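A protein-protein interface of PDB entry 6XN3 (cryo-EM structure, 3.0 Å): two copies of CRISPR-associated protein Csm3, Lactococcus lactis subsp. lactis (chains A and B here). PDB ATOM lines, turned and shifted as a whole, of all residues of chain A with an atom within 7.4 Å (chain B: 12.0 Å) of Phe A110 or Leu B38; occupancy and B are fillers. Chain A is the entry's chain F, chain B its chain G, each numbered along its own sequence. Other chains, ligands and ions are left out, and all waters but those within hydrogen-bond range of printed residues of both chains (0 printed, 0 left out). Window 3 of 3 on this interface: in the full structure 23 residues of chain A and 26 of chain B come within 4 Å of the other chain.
N of Val A112 lies within hydrogen-bond range of O of Leu A107 (3.3 Å).
The backbone carbonyl oxygen (O) of Ile A139 lies within hydrogen-bond range of the side-chain hydroxyl (OG) of Ser A142, at 3.2 Å.
The side-chain carboxylate (OD2) of Asp B36 sits at hydrogen-bond distance from the backbone NH (N) of Thr B39, at 3.5 Å.
O of Leu B41 is in hydrogen-bond range of N of Asp B36, at 3.0 Å.
The side-chain amino group of Lys B100 is in salt-bridge range of the side-chain carboxylate of Asp B36.
Among the printed residues, pairs that only touch across the chains: Leu A107 with Leu B38 (3.7 Å), Phe A110 with Leu B38 (3.7 Å), Val A112 with Thr B37 (3.4 Å), Glu A116 with Thr B37 (3.7 Å), Ile A139 with Thr B37 (3.3 Å), Ala A140 with Asp B36 (3.4 Å) and Ala A140 with Leu B38 (3.96 Å).
Position printed for both chains: 104.
Of the 7 pairs that touch across the chains among the printed residues, none has its exchanged pair printed and touching as well.
Of the 17 printed residues of chain A, 6 touch a printed residue of chain B.
Along chain A the printed residues that touch a printed residue of chain B span positions 107 to 140.
Of the 16 printed residues of chain B, 3 touch a printed residue of chain A.
Printed residues of chain B that touch a printed residue of chain A: Asp B36, Thr B37 and Leu B38.
Hydrophobic or aromatic side chains of chain B within 4 Å of the printed part of chain A: Leu B38.
Leu B38 touches three residues of chain A.
No residue of chain B comes within 4 Å of Glu A106.
Leu A107 touches just one residue of chain B: Leu B38 (3.7 Å).
No residue of chain B comes within 4 Å of Glu A108.
No residue of chain B comes within 4 Å of Thr A109.
No residue of chain B comes within 4 Å of Asn A111.
Of chain B, only Thr B37 (3.4 Å) comes within 4 Å of Val A112.
Ile A139 touches just one residue of chain B: Thr B37.
Printed residues of chain B within 4 Å of Glu A116: Thr B37 (3.7 Å).
Of the printed residues of chain A, Thr B37 touches Val A112 (3.4 Å), Glu A116 (3.7 Å) and Ile A139 (3.3 Å).
Printed residues of chain A within 4 Å of Asp B36: Ala A140 (3.4 Å).
Thr B39 touches none of the printed residues of chain A.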
ATOM      1  N   ASN A 103     -27.739 -32.679  -9.147  1.00  0.00           N
ATOM      2  CA  ASN A 103     -28.327 -31.883  -8.081  1.00  0.00           C
ATOM      3  C   ASN A 103     -27.734 -30.484  -7.982  1.00  0.00           C
ATOM      4  O   ASN A 103     -27.650 -29.932  -6.879  1.00  0.00           O
ATOM      5  CB  ASN A 103     -28.198 -32.623  -6.751  1.00  0.00           C
ATOM      6  CG  ASN A 103     -26.771 -32.772  -6.307  1.00  0.00           C
ATOM      7  OD1 ASN A 103     -25.872 -32.904  -7.125  1.00  0.00           O
ATOM      8  ND2 ASN A 103     -26.553 -32.747  -5.003  1.00  0.00           N
ATOM      9  N   LEU A 104     -27.351 -29.878  -9.111  1.00  0.00           N
ATOM     10  CA  LEU A 104     -26.895 -28.489  -9.092  1.00  0.00           C
ATOM     11  C   LEU A 104     -28.018 -27.538  -8.691  1.00  0.00           C
ATOM     12  O   LEU A 104     -27.754 -26.449  -8.171  1.00  0.00           O
ATOM     13  CB  LEU A 104     -26.336 -28.097 -10.458  1.00  0.00           C
ATOM     14  CG  LEU A 104     -25.471 -26.836 -10.483  1.00  0.00           C
ATOM     15  CD1 LEU A 104     -24.155 -27.090  -9.797  1.00  0.00           C
ATOM     16  CD2 LEU A 104     -25.263 -26.321 -11.887  1.00  0.00           C
ATOM     17  N   ALA A 105     -29.272 -27.934  -8.919  1.00  0.00           N
ATOM     18  CA  ALA A 105     -30.395 -27.201  -8.352  1.00  0.00           C
ATOM     19  C   ALA A 105     -30.393 -27.281  -6.832  1.00  0.00           C
ATOM     20  O   ALA A 105     -30.757 -26.316  -6.152  1.00  0.00           O
ATOM     21  CB  ALA A 105     -31.708 -27.739  -8.913  1.00  0.00           C
ATOM     22  N   GLU A 106     -29.994 -28.428  -6.278  1.00  0.00           N
ATOM     23  CA  GLU A 106     -29.909 -28.551  -4.827  1.00  0.00           C
ATOM     24  C   GLU A 106     -28.655 -27.876  -4.283  1.00  0.00           C
ATOM     25  O   GLU A 106     -28.680 -27.295  -3.193  1.00  0.00           O
ATOM     26  CB  GLU A 106     -29.950 -30.024  -4.426  1.00  0.00           C
ATOM     27  CG  GLU A 106     -29.955 -30.269  -2.930  1.00  0.00           C
ATOM     28  CD  GLU A 106     -29.967 -31.741  -2.581  1.00  0.00           C
ATOM     29  OE1 GLU A 106     -29.654 -32.081  -1.422  1.00  0.00           O
ATOM     30  OE2 GLU A 106     -30.294 -32.557  -3.467  1.00  0.00           O
ATOM     31  N   LEU A 107     -27.549 -27.927  -5.022  1.00  0.00           N
ATOM     32  CA  LEU A 107     -26.332 -27.296  -4.525  1.00  0.00           C
ATOM     33  C   LEU A 107     -26.381 -25.784  -4.690  1.00  0.00           C
ATOM     34  O   LEU A 107     -25.594 -25.066  -4.069  1.00  0.00           O
ATOM     35  CB  LEU A 107     -25.100 -27.860  -5.226  1.00  0.00           C
ATOM     36  CG  LEU A 107     -24.854 -29.362  -5.145  1.00  0.00           C
ATOM     37  CD1 LEU A 107     -23.555 -29.699  -5.816  1.00  0.00           C
ATOM     38  CD2 LEU A 107     -24.845 -29.838  -3.721  1.00  0.00           C
ATOM     39  N   GLU A 108     -27.280 -25.281  -5.535  1.00  0.00           N
ATOM     40  CA  GLU A 108     -27.495 -23.839  -5.584  1.00  0.00           C
ATOM     41  C   GLU A 108     -28.284 -23.363  -4.374  1.00  0.00           C
ATOM     42  O   GLU A 108     -28.063 -22.250  -3.884  1.00  0.00           O
ATOM     43  CB  GLU A 108     -28.200 -23.455  -6.888  1.00  0.00           C
ATOM     44  CG  GLU A 108     -28.446 -21.961  -7.085  1.00  0.00           C
ATOM     45  CD  GLU A 108     -27.168 -21.146  -7.221  1.00  0.00           C
ATOM     46  OE1 GLU A 108     -26.131 -21.699  -7.647  1.00  0.00           O
ATOM     47  OE2 GLU A 108     -27.205 -19.940  -6.893  1.00  0.00           O
ATOM     48  N   THR A 109     -29.195 -24.203  -3.877  1.00  0.00           N
ATOM     49  CA  THR A 109     -29.956 -23.912  -2.670  1.00  0.00           C
ATOM     50  C   THR A 109     -29.050 -23.743  -1.458  1.00  0.00           C
ATOM     51  O   THR A 109     -29.264 -22.830  -0.654  1.00  0.00           O
ATOM     52  CB  THR A 109     -30.976 -25.034  -2.445  1.00  0.00           C
ATOM     53  OG1 THR A 109     -31.960 -24.989  -3.483  1.00  0.00           O
ATOM     54  CG2 THR A 109     -31.678 -24.911  -1.107  1.00  0.00           C
ATOM     55  N   PHE A 110     -27.991 -24.538  -1.362  1.00  0.00           N
ATOM     56  CA  PHE A 110     -27.031 -24.436  -0.274  1.00  0.00           C
ATOM     57  C   PHE A 110     -26.016 -23.327  -0.507  1.00  0.00           C
ATOM     58  O   PHE A 110     -25.141 -23.126   0.339  1.00  0.00           O
ATOM     59  CB  PHE A 110     -26.302 -25.767  -0.073  1.00  0.00           C
ATOM     60  CG  PHE A 110     -27.089 -26.794   0.695  1.00  0.00           C
ATOM     61  CD1 PHE A 110     -28.307 -27.263   0.230  1.00  0.00           C
ATOM     62  CD2 PHE A 110     -26.604 -27.292   1.889  1.00  0.00           C
ATOM     63  CE1 PHE A 110     -29.020 -28.206   0.936  1.00  0.00           C
ATOM     64  CE2 PHE A 110     -27.314 -28.237   2.601  1.00  0.00           C
ATOM     65  CZ  PHE A 110     -28.525 -28.693   2.121  1.00  0.00           C
ATOM     66  N   ASN A 111     -26.109 -22.636  -1.645  1.00  0.00           N
ATOM     67  CA  ASN A 111     -25.307 -21.466  -2.011  1.00  0.00           C
ATOM     68  C   ASN A 111     -23.815 -21.784  -2.018  1.00  0.00           C
ATOM     69  O   ASN A 111     -22.988 -21.076  -1.447  1.00  0.00           O
ATOM     70  CB  ASN A 111     -25.622 -20.280  -1.099  1.00  0.00           C
ATOM     71  CG  ASN A 111     -27.033 -19.770  -1.286  1.00  0.00           C
ATOM     72  OD1 ASN A 111     -27.950 -20.165  -0.570  1.00  0.00           O
ATOM     73  ND2 ASN A 111     -27.217 -18.894  -2.265  1.00  0.00           N
ATOM     74  N   VAL A 112     -23.487 -22.881  -2.696  1.00  0.00           N
ATOM     75  CA  VAL A 112     -22.115 -23.347  -2.792  1.00  0.00           C
ATOM     76  C   VAL A 112     -21.930 -23.905  -4.194  1.00  0.00           C
ATOM     77  O   VAL A 112     -22.867 -24.441  -4.790  1.00  0.00           O
ATOM     78  CB  VAL A 112     -21.810 -24.387  -1.681  1.00  0.00           C
ATOM     79  CG1 VAL A 112     -22.765 -25.569  -1.742  1.00  0.00           C
ATOM     80  CG2 VAL A 112     -20.355 -24.833  -1.686  1.00  0.00           C
ATOM     81  N   SER A 113     -20.732 -23.731  -4.743  1.00  0.00           N
ATOM     82  CA  SER A 113     -20.390 -24.336  -6.017  1.00  0.00           C
ATOM     83  C   SER A 113     -20.336 -25.856  -5.883  1.00  0.00           C
ATOM     84  O   SER A 113     -20.273 -26.413  -4.788  1.00  0.00           O
ATOM     85  CB  SER A 113     -19.053 -23.800  -6.518  1.00  0.00           C
ATOM     86  OG  SER A 113     -18.513 -24.638  -7.520  1.00  0.00           O
ATOM     87  N   GLU A 116     -14.582 -27.744  -5.479  1.00  0.00           N
ATOM     88  CA  GLU A 116     -13.781 -27.092  -4.454  1.00  0.00           C
ATOM     89  C   GLU A 116     -12.316 -27.348  -4.759  1.00  0.00           C
ATOM     90  O   GLU A 116     -11.977 -28.088  -5.682  1.00  0.00           O
ATOM     91  CB  GLU A 116     -14.139 -27.605  -3.062  1.00  0.00           C
ATOM     92  CG  GLU A 116     -13.890 -29.085  -2.901  1.00  0.00           C
ATOM     93  CD  GLU A 116     -13.591 -29.485  -1.479  1.00  0.00           C
ATOM     94  OE1 GLU A 116     -13.561 -28.596  -0.603  1.00  0.00           O
ATOM     95  OE2 GLU A 116     -13.376 -30.690  -1.239  1.00  0.00           O
ATOM     96  N   ILE A 139     -17.342 -31.508  -4.444  1.00  0.00           N
ATOM     97  CA  ILE A 139     -17.657 -31.450  -3.030  1.00  0.00           C
ATOM     98  C   ILE A 139     -18.447 -32.688  -2.639  1.00  0.00           C
ATOM     99  O   ILE A 139     -18.952 -33.433  -3.480  1.00  0.00           O
ATOM    100  CB  ILE A 139     -18.435 -30.178  -2.680  1.00  0.00           C
ATOM    101  CG1 ILE A 139     -19.766 -30.174  -3.407  1.00  0.00           C
ATOM    102  CG2 ILE A 139     -17.656 -28.979  -3.131  1.00  0.00           C
ATOM    103  CD1 ILE A 139     -20.682 -29.090  -2.936  1.00  0.00           C
ATOM    104  N   ALA A 140     -18.560 -32.906  -1.339  1.00  0.00           N
ATOM    105  CA  ALA A 140     -19.419 -33.971  -0.867  1.00  0.00           C
ATOM    106  C   ALA A 140     -20.880 -33.556  -0.994  1.00  0.00           C
ATOM    107  O   ALA A 140     -21.207 -32.394  -1.233  1.00  0.00           O
ATOM    108  CB  ALA A 140     -19.088 -34.329   0.577  1.00  0.00           C
ATOM    109  N   GLY A 141     -21.769 -34.531  -0.843  1.00  0.00           N
ATOM    110  CA  GLY A 141     -23.183 -34.245  -0.943  1.00  0.00           C
ATOM    111  C   GLY A 141     -23.692 -34.037  -2.347  1.00  0.00           C
ATOM    112  O   GLY A 141     -24.803 -33.540  -2.524  1.00  0.00           O
ATOM    113  N   SER A 142     -22.914 -34.403  -3.355  1.00  0.00           N
ATOM    114  CA  SER A 142     -23.330 -34.296  -4.742  1.00  0.00           C
ATOM    115  C   SER A 142     -24.054 -35.568  -5.150  1.00  0.00           C
ATOM    116  O   SER A 142     -23.754 -36.650  -4.645  1.00  0.00           O
ATOM    117  CB  SER A 142     -22.129 -34.067  -5.655  1.00  0.00           C
ATOM    118  OG  SER A 142     -21.503 -32.836  -5.364  1.00  0.00           O
ATOM    119  N   LYS A 143     -25.018 -35.432  -6.049  1.00  0.00           N
ATOM    120  CA  LYS A 143     -25.747 -36.566  -6.593  1.00  0.00           C
ATOM    121  C   LYS A 143     -25.349 -36.780  -8.045  1.00  0.00           C
ATOM    122  O   LYS A 143     -24.839 -35.878  -8.708  1.00  0.00           O
ATOM    123  CB  LYS A 143     -27.258 -36.351  -6.490  1.00  0.00           C
ATOM    124  CG  LYS A 143     -27.884 -36.815  -5.191  1.00  0.00           C
ATOM    125  CD  LYS A 143     -27.713 -35.801  -4.088  1.00  0.00           C
ATOM    126  CE  LYS A 143     -28.385 -36.261  -2.814  1.00  0.00           C
ATOM    127  NZ  LYS A 143     -28.156 -35.301  -1.700  1.00  0.00           N
ATOM    128  N   VAL B  33      -9.591 -22.841   8.911  1.00  0.00           N
ATOM    129  CA  VAL B  33      -9.468 -24.290   8.916  1.00  0.00           C
ATOM    130  C   VAL B  33     -10.231 -24.862   7.732  1.00  0.00           C
ATOM    131  O   VAL B  33     -11.106 -24.213   7.154  1.00  0.00           O
ATOM    132  CB  VAL B  33      -9.970 -24.875  10.246  1.00  0.00           C
ATOM    133  CG1 VAL B  33      -9.118 -24.371  11.371  1.00  0.00           C
ATOM    134  CG2 VAL B  33     -11.404 -24.491  10.469  1.00  0.00           C
ATOM    135  N   VAL B  34      -9.886 -26.092   7.359  1.00  0.00           N
ATOM    136  CA  VAL B  34     -10.541 -26.745   6.237  1.00  0.00           C
ATOM    137  C   VAL B  34     -11.925 -27.214   6.669  1.00  0.00           C
ATOM    138  O   VAL B  34     -12.153 -27.567   7.835  1.00  0.00           O
ATOM    139  CB  VAL B  34      -9.652 -27.884   5.697  1.00  0.00           C
ATOM    140  CG1 VAL B  34      -9.567 -29.047   6.654  1.00  0.00           C
ATOM    141  CG2 VAL B  34     -10.114 -28.355   4.332  1.00  0.00           C
ATOM    142  N   ARG B  35     -12.881 -27.149   5.747  1.00  0.00           N
ATOM    143  CA  ARG B  35     -14.267 -27.453   6.053  1.00  0.00           C
ATOM    144  C   ARG B  35     -14.866 -28.266   4.922  1.00  0.00           C
ATOM    145  O   ARG B  35     -14.329 -28.319   3.814  1.00  0.00           O
ATOM    146  CB  ARG B  35     -15.090 -26.182   6.255  1.00  0.00           C
ATOM    147  CG  ARG B  35     -14.837 -25.449   7.546  1.00  0.00           C
ATOM    148  CD  ARG B  35     -15.492 -24.091   7.504  1.00  0.00           C
ATOM    149  NE  ARG B  35     -15.354 -23.374   8.761  1.00  0.00           N
ATOM    150  CZ  ARG B  35     -16.245 -23.422   9.742  1.00  0.00           C
ATOM    151  NH1 ARG B  35     -17.332 -24.159   9.617  1.00  0.00           N
ATOM    152  NH2 ARG B  35     -16.045 -22.737  10.850  1.00  0.00           N
ATOM    153  N   ASP B  36     -15.996 -28.900   5.208  1.00  0.00           N
ATOM    154  CA  ASP B  36     -16.793 -29.568   4.188  1.00  0.00           C
ATOM    155  C   ASP B  36     -17.782 -28.557   3.635  1.00  0.00           C
ATOM    156  O   ASP B  36     -18.787 -28.257   4.279  1.00  0.00           O
ATOM    157  CB  ASP B  36     -17.519 -30.776   4.764  1.00  0.00           C
ATOM    158  CG  ASP B  36     -18.536 -31.344   3.804  1.00  0.00           C
ATOM    159  OD1 ASP B  36     -18.129 -31.970   2.804  1.00  0.00           O
ATOM    160  OD2 ASP B  36     -19.744 -31.162   4.044  1.00  0.00           O
ATOM    161  N   THR B  37     -17.528 -28.081   2.413  1.00  0.00           N
ATOM    162  CA  THR B  37     -18.069 -26.797   1.973  1.00  0.00           C
ATOM    163  C   THR B  37     -19.569 -26.832   1.715  1.00  0.00           C
ATOM    164  O   THR B  37     -20.186 -25.775   1.560  1.00  0.00           O
ATOM    165  CB  THR B  37     -17.338 -26.335   0.723  1.00  0.00           C
ATOM    166  OG1 THR B  37     -17.544 -27.295  -0.314  1.00  0.00           O
ATOM    167  CG2 THR B  37     -15.848 -26.210   0.999  1.00  0.00           C
ATOM    168  N   LEU B  38     -20.176 -28.015   1.652  1.00  0.00           N
ATOM    169  CA  LEU B  38     -21.632 -28.073   1.649  1.00  0.00           C
ATOM    170  C   LEU B  38     -22.193 -27.673   3.003  1.00  0.00           C
ATOM    171  O   LEU B  38     -23.101 -26.841   3.092  1.00  0.00           O
ATOM    172  CB  LEU B  38     -22.115 -29.471   1.277  1.00  0.00           C
ATOM    173  CG  LEU B  38     -23.637 -29.534   1.183  1.00  0.00           C
ATOM    174  CD1 LEU B  38     -24.084 -29.061  -0.176  1.00  0.00           C
ATOM    175  CD2 LEU B  38     -24.162 -30.931   1.473  1.00  0.00           C
ATOM    176  N   THR B  39     -21.666 -28.255   4.067  1.00  0.00           N
ATOM    177  CA  THR B  39     -22.106 -27.921   5.409  1.00  0.00           C
ATOM    178  C   THR B  39     -21.337 -26.737   5.984  1.00  0.00           C
ATOM    179  O   THR B  39     -21.924 -25.925   6.710  1.00  0.00           O
ATOM    180  CB  THR B  39     -21.954 -29.157   6.299  1.00  0.00           C
ATOM    181  OG1 THR B  39     -22.698 -30.231   5.726  1.00  0.00           O
ATOM    182  CG2 THR B  39     -22.535 -28.911   7.671  1.00  0.00           C
ATOM    183  N   ARG B  40     -20.086 -26.561   5.569  1.00  0.00           N
ATOM    184  CA  ARG B  40     -19.094 -25.722   6.242  1.00  0.00           C
ATOM    185  C   ARG B  40     -19.059 -26.038   7.730  1.00  0.00           C
ATOM    186  O   ARG B  40     -19.242 -25.189   8.599  1.00  0.00           O
ATOM    187  CB  ARG B  40     -19.285 -24.236   5.935  1.00  0.00           C
ATOM    188  CG  ARG B  40     -18.943 -23.933   4.470  1.00  0.00           C
ATOM    189  CD  ARG B  40     -18.899 -22.457   4.106  1.00  0.00           C
ATOM    190  NE  ARG B  40     -20.178 -21.769   4.228  1.00  0.00           N
ATOM    191  CZ  ARG B  40     -21.084 -21.698   3.255  1.00  0.00           C
ATOM    192  NH1 ARG B  40     -20.852 -22.286   2.088  1.00  0.00           N
ATOM    193  NH2 ARG B  40     -22.220 -21.040   3.447  1.00  0.00           N
ATOM    194  N   LEU B  41     -18.818 -27.317   7.987  1.00  0.00           N
ATOM    195  CA  LEU B  41     -18.489 -27.992   9.216  1.00  0.00           C
ATOM    196  C   LEU B  41     -16.996 -28.261   9.220  1.00  0.00           C
ATOM    197  O   LEU B  41     -16.457 -28.648   8.182  1.00  0.00           O
ATOM    198  CB  LEU B  41     -19.240 -29.310   9.300  1.00  0.00           C
ATOM    199  CG  LEU B  41     -19.670 -29.802  10.660  1.00  0.00           C
ATOM    200  CD1 LEU B  41     -20.548 -28.766  11.282  1.00  0.00           C
ATOM    201  CD2 LEU B  41     -20.441 -31.068  10.456  1.00  0.00           C
ATOM    202  N   PRO B  42     -16.299 -28.033  10.332  1.00  0.00           N
ATOM    203  CA  PRO B  42     -14.840 -28.202  10.344  1.00  0.00           C
ATOM    204  C   PRO B  42     -14.437 -29.653  10.135  1.00  0.00           C
ATOM    205  O   PRO B  42     -15.124 -30.577  10.574  1.00  0.00           O
ATOM    206  CB  PRO B  42     -14.434 -27.689  11.726  1.00  0.00           C
ATOM    207  CG  PRO B  42     -15.664 -27.659  12.510  1.00  0.00           C
ATOM    208  CD  PRO B  42     -16.788 -27.437  11.580  1.00  0.00           C
ATOM    209  N   LEU B  43     -13.317 -29.843   9.446  1.00  0.00           N
ATOM    210  CA  LEU B  43     -12.996 -31.104   8.801  1.00  0.00           C
ATOM    211  C   LEU B  43     -11.599 -31.568   9.176  1.00  0.00           C
ATOM    212  O   LEU B  43     -10.670 -30.766   9.282  1.00  0.00           O
ATOM    213  CB  LEU B  43     -13.084 -30.956   7.282  1.00  0.00           C
ATOM    214  CG  LEU B  43     -13.014 -32.196   6.397  1.00  0.00           C
ATOM    215  CD1 LEU B  43     -14.373 -32.819   6.278  1.00  0.00           C
ATOM    216  CD2 LEU B  43     -12.465 -31.847   5.030  1.00  0.00           C
ATOM    217  N   ASP B  98     -12.252 -38.737   4.867  1.00  0.00           N
ATOM    218  CA  ASP B  98     -12.427 -37.379   5.349  1.00  0.00           C
ATOM    219  C   ASP B  98     -13.345 -37.397   6.559  1.00  0.00           C
ATOM    220  O   ASP B  98     -14.491 -37.846   6.472  1.00  0.00           O
ATOM    221  CB  ASP B  98     -13.008 -36.511   4.242  1.00  0.00           C
ATOM    222  CG  ASP B  98     -11.941 -35.930   3.344  1.00  0.00           C
ATOM    223  OD1 ASP B  98     -10.761 -36.284   3.526  1.00  0.00           O
ATOM    224  OD2 ASP B  98     -12.279 -35.129   2.449  1.00  0.00           O
ATOM    225  N   ILE B  99     -12.841 -36.922   7.690  1.00  0.00           N
ATOM    226  CA  ILE B  99     -13.563 -36.979   8.951  1.00  0.00           C
ATOM    227  C   ILE B  99     -14.285 -35.660   9.162  1.00  0.00           C
ATOM    228  O   ILE B  99     -13.684 -34.587   9.034  1.00  0.00           O
ATOM    229  CB  ILE B  99     -12.616 -37.279  10.120  1.00  0.00           C
ATOM    230  CG1 ILE B  99     -11.570 -38.305   9.707  1.00  0.00           C
ATOM    231  CG2 ILE B  99     -13.391 -37.803  11.276  1.00  0.00           C
ATOM    232  CD1 ILE B  99     -10.460 -38.448  10.689  1.00  0.00           C
ATOM    233  N   LYS B 100     -15.571 -35.736   9.477  1.00  0.00           N
ATOM    234  CA  LYS B 100     -16.378 -34.561   9.757  1.00  0.00           C
ATOM    235  C   LYS B 100     -16.676 -34.484  11.246  1.00  0.00           C
ATOM    236  O   LYS B 100     -16.686 -35.499  11.943  1.00  0.00           O
ATOM    237  CB  LYS B 100     -17.684 -34.586   8.966  1.00  0.00           C
ATOM    238  CG  LYS B 100     -17.520 -34.274   7.499  1.00  0.00           C
ATOM    239  CD  LYS B 100     -18.698 -34.759   6.685  1.00  0.00           C
ATOM    240  CE  LYS B 100     -19.874 -33.823   6.817  1.00  0.00           C
ATOM    241  NZ  LYS B 100     -21.020 -34.271   5.987  1.00  0.00           N
ATOM    242  N   LEU B 101     -16.901 -33.266  11.728  1.00  0.00           N
ATOM    243  CA  LEU B 101     -17.236 -33.068  13.130  1.00  0.00           C
ATOM    244  C   LEU B 101     -18.620 -33.628  13.420  1.00  0.00           C
ATOM    245  O   LEU B 101     -19.571 -33.398  12.673  1.00  0.00           O
ATOM    246  CB  LEU B 101     -17.167 -31.583  13.477  1.00  0.00           C
ATOM    247  CG  LEU B 101     -17.310 -31.159  14.933  1.00  0.00           C
ATOM    248  CD1 LEU B 101     -16.330 -30.071  15.205  1.00  0.00           C
ATOM    249  CD2 LEU B 101     -18.686 -30.627  15.202  1.00  0.00           C
ATOM    250  N   LEU B 104     -21.580 -31.507  16.938  1.00  0.00           N
ATOM    251  CA  LEU B 104     -22.073 -30.136  16.836  1.00  0.00           C
ATOM    252  C   LEU B 104     -23.345 -29.929  17.652  1.00  0.00           C
ATOM    253  O   LEU B 104     -23.605 -28.819  18.117  1.00  0.00           O
ATOM    254  CB  LEU B 104     -22.315 -29.777  15.373  1.00  0.00           C
ATOM    255  CG  LEU B 104     -22.780 -28.357  15.056  1.00  0.00           C
ATOM    256  CD1 LEU B 104     -21.645 -27.377  15.251  1.00  0.00           C
ATOM    257  CD2 LEU B 104     -23.371 -28.267  13.667  1.00  0.00           C
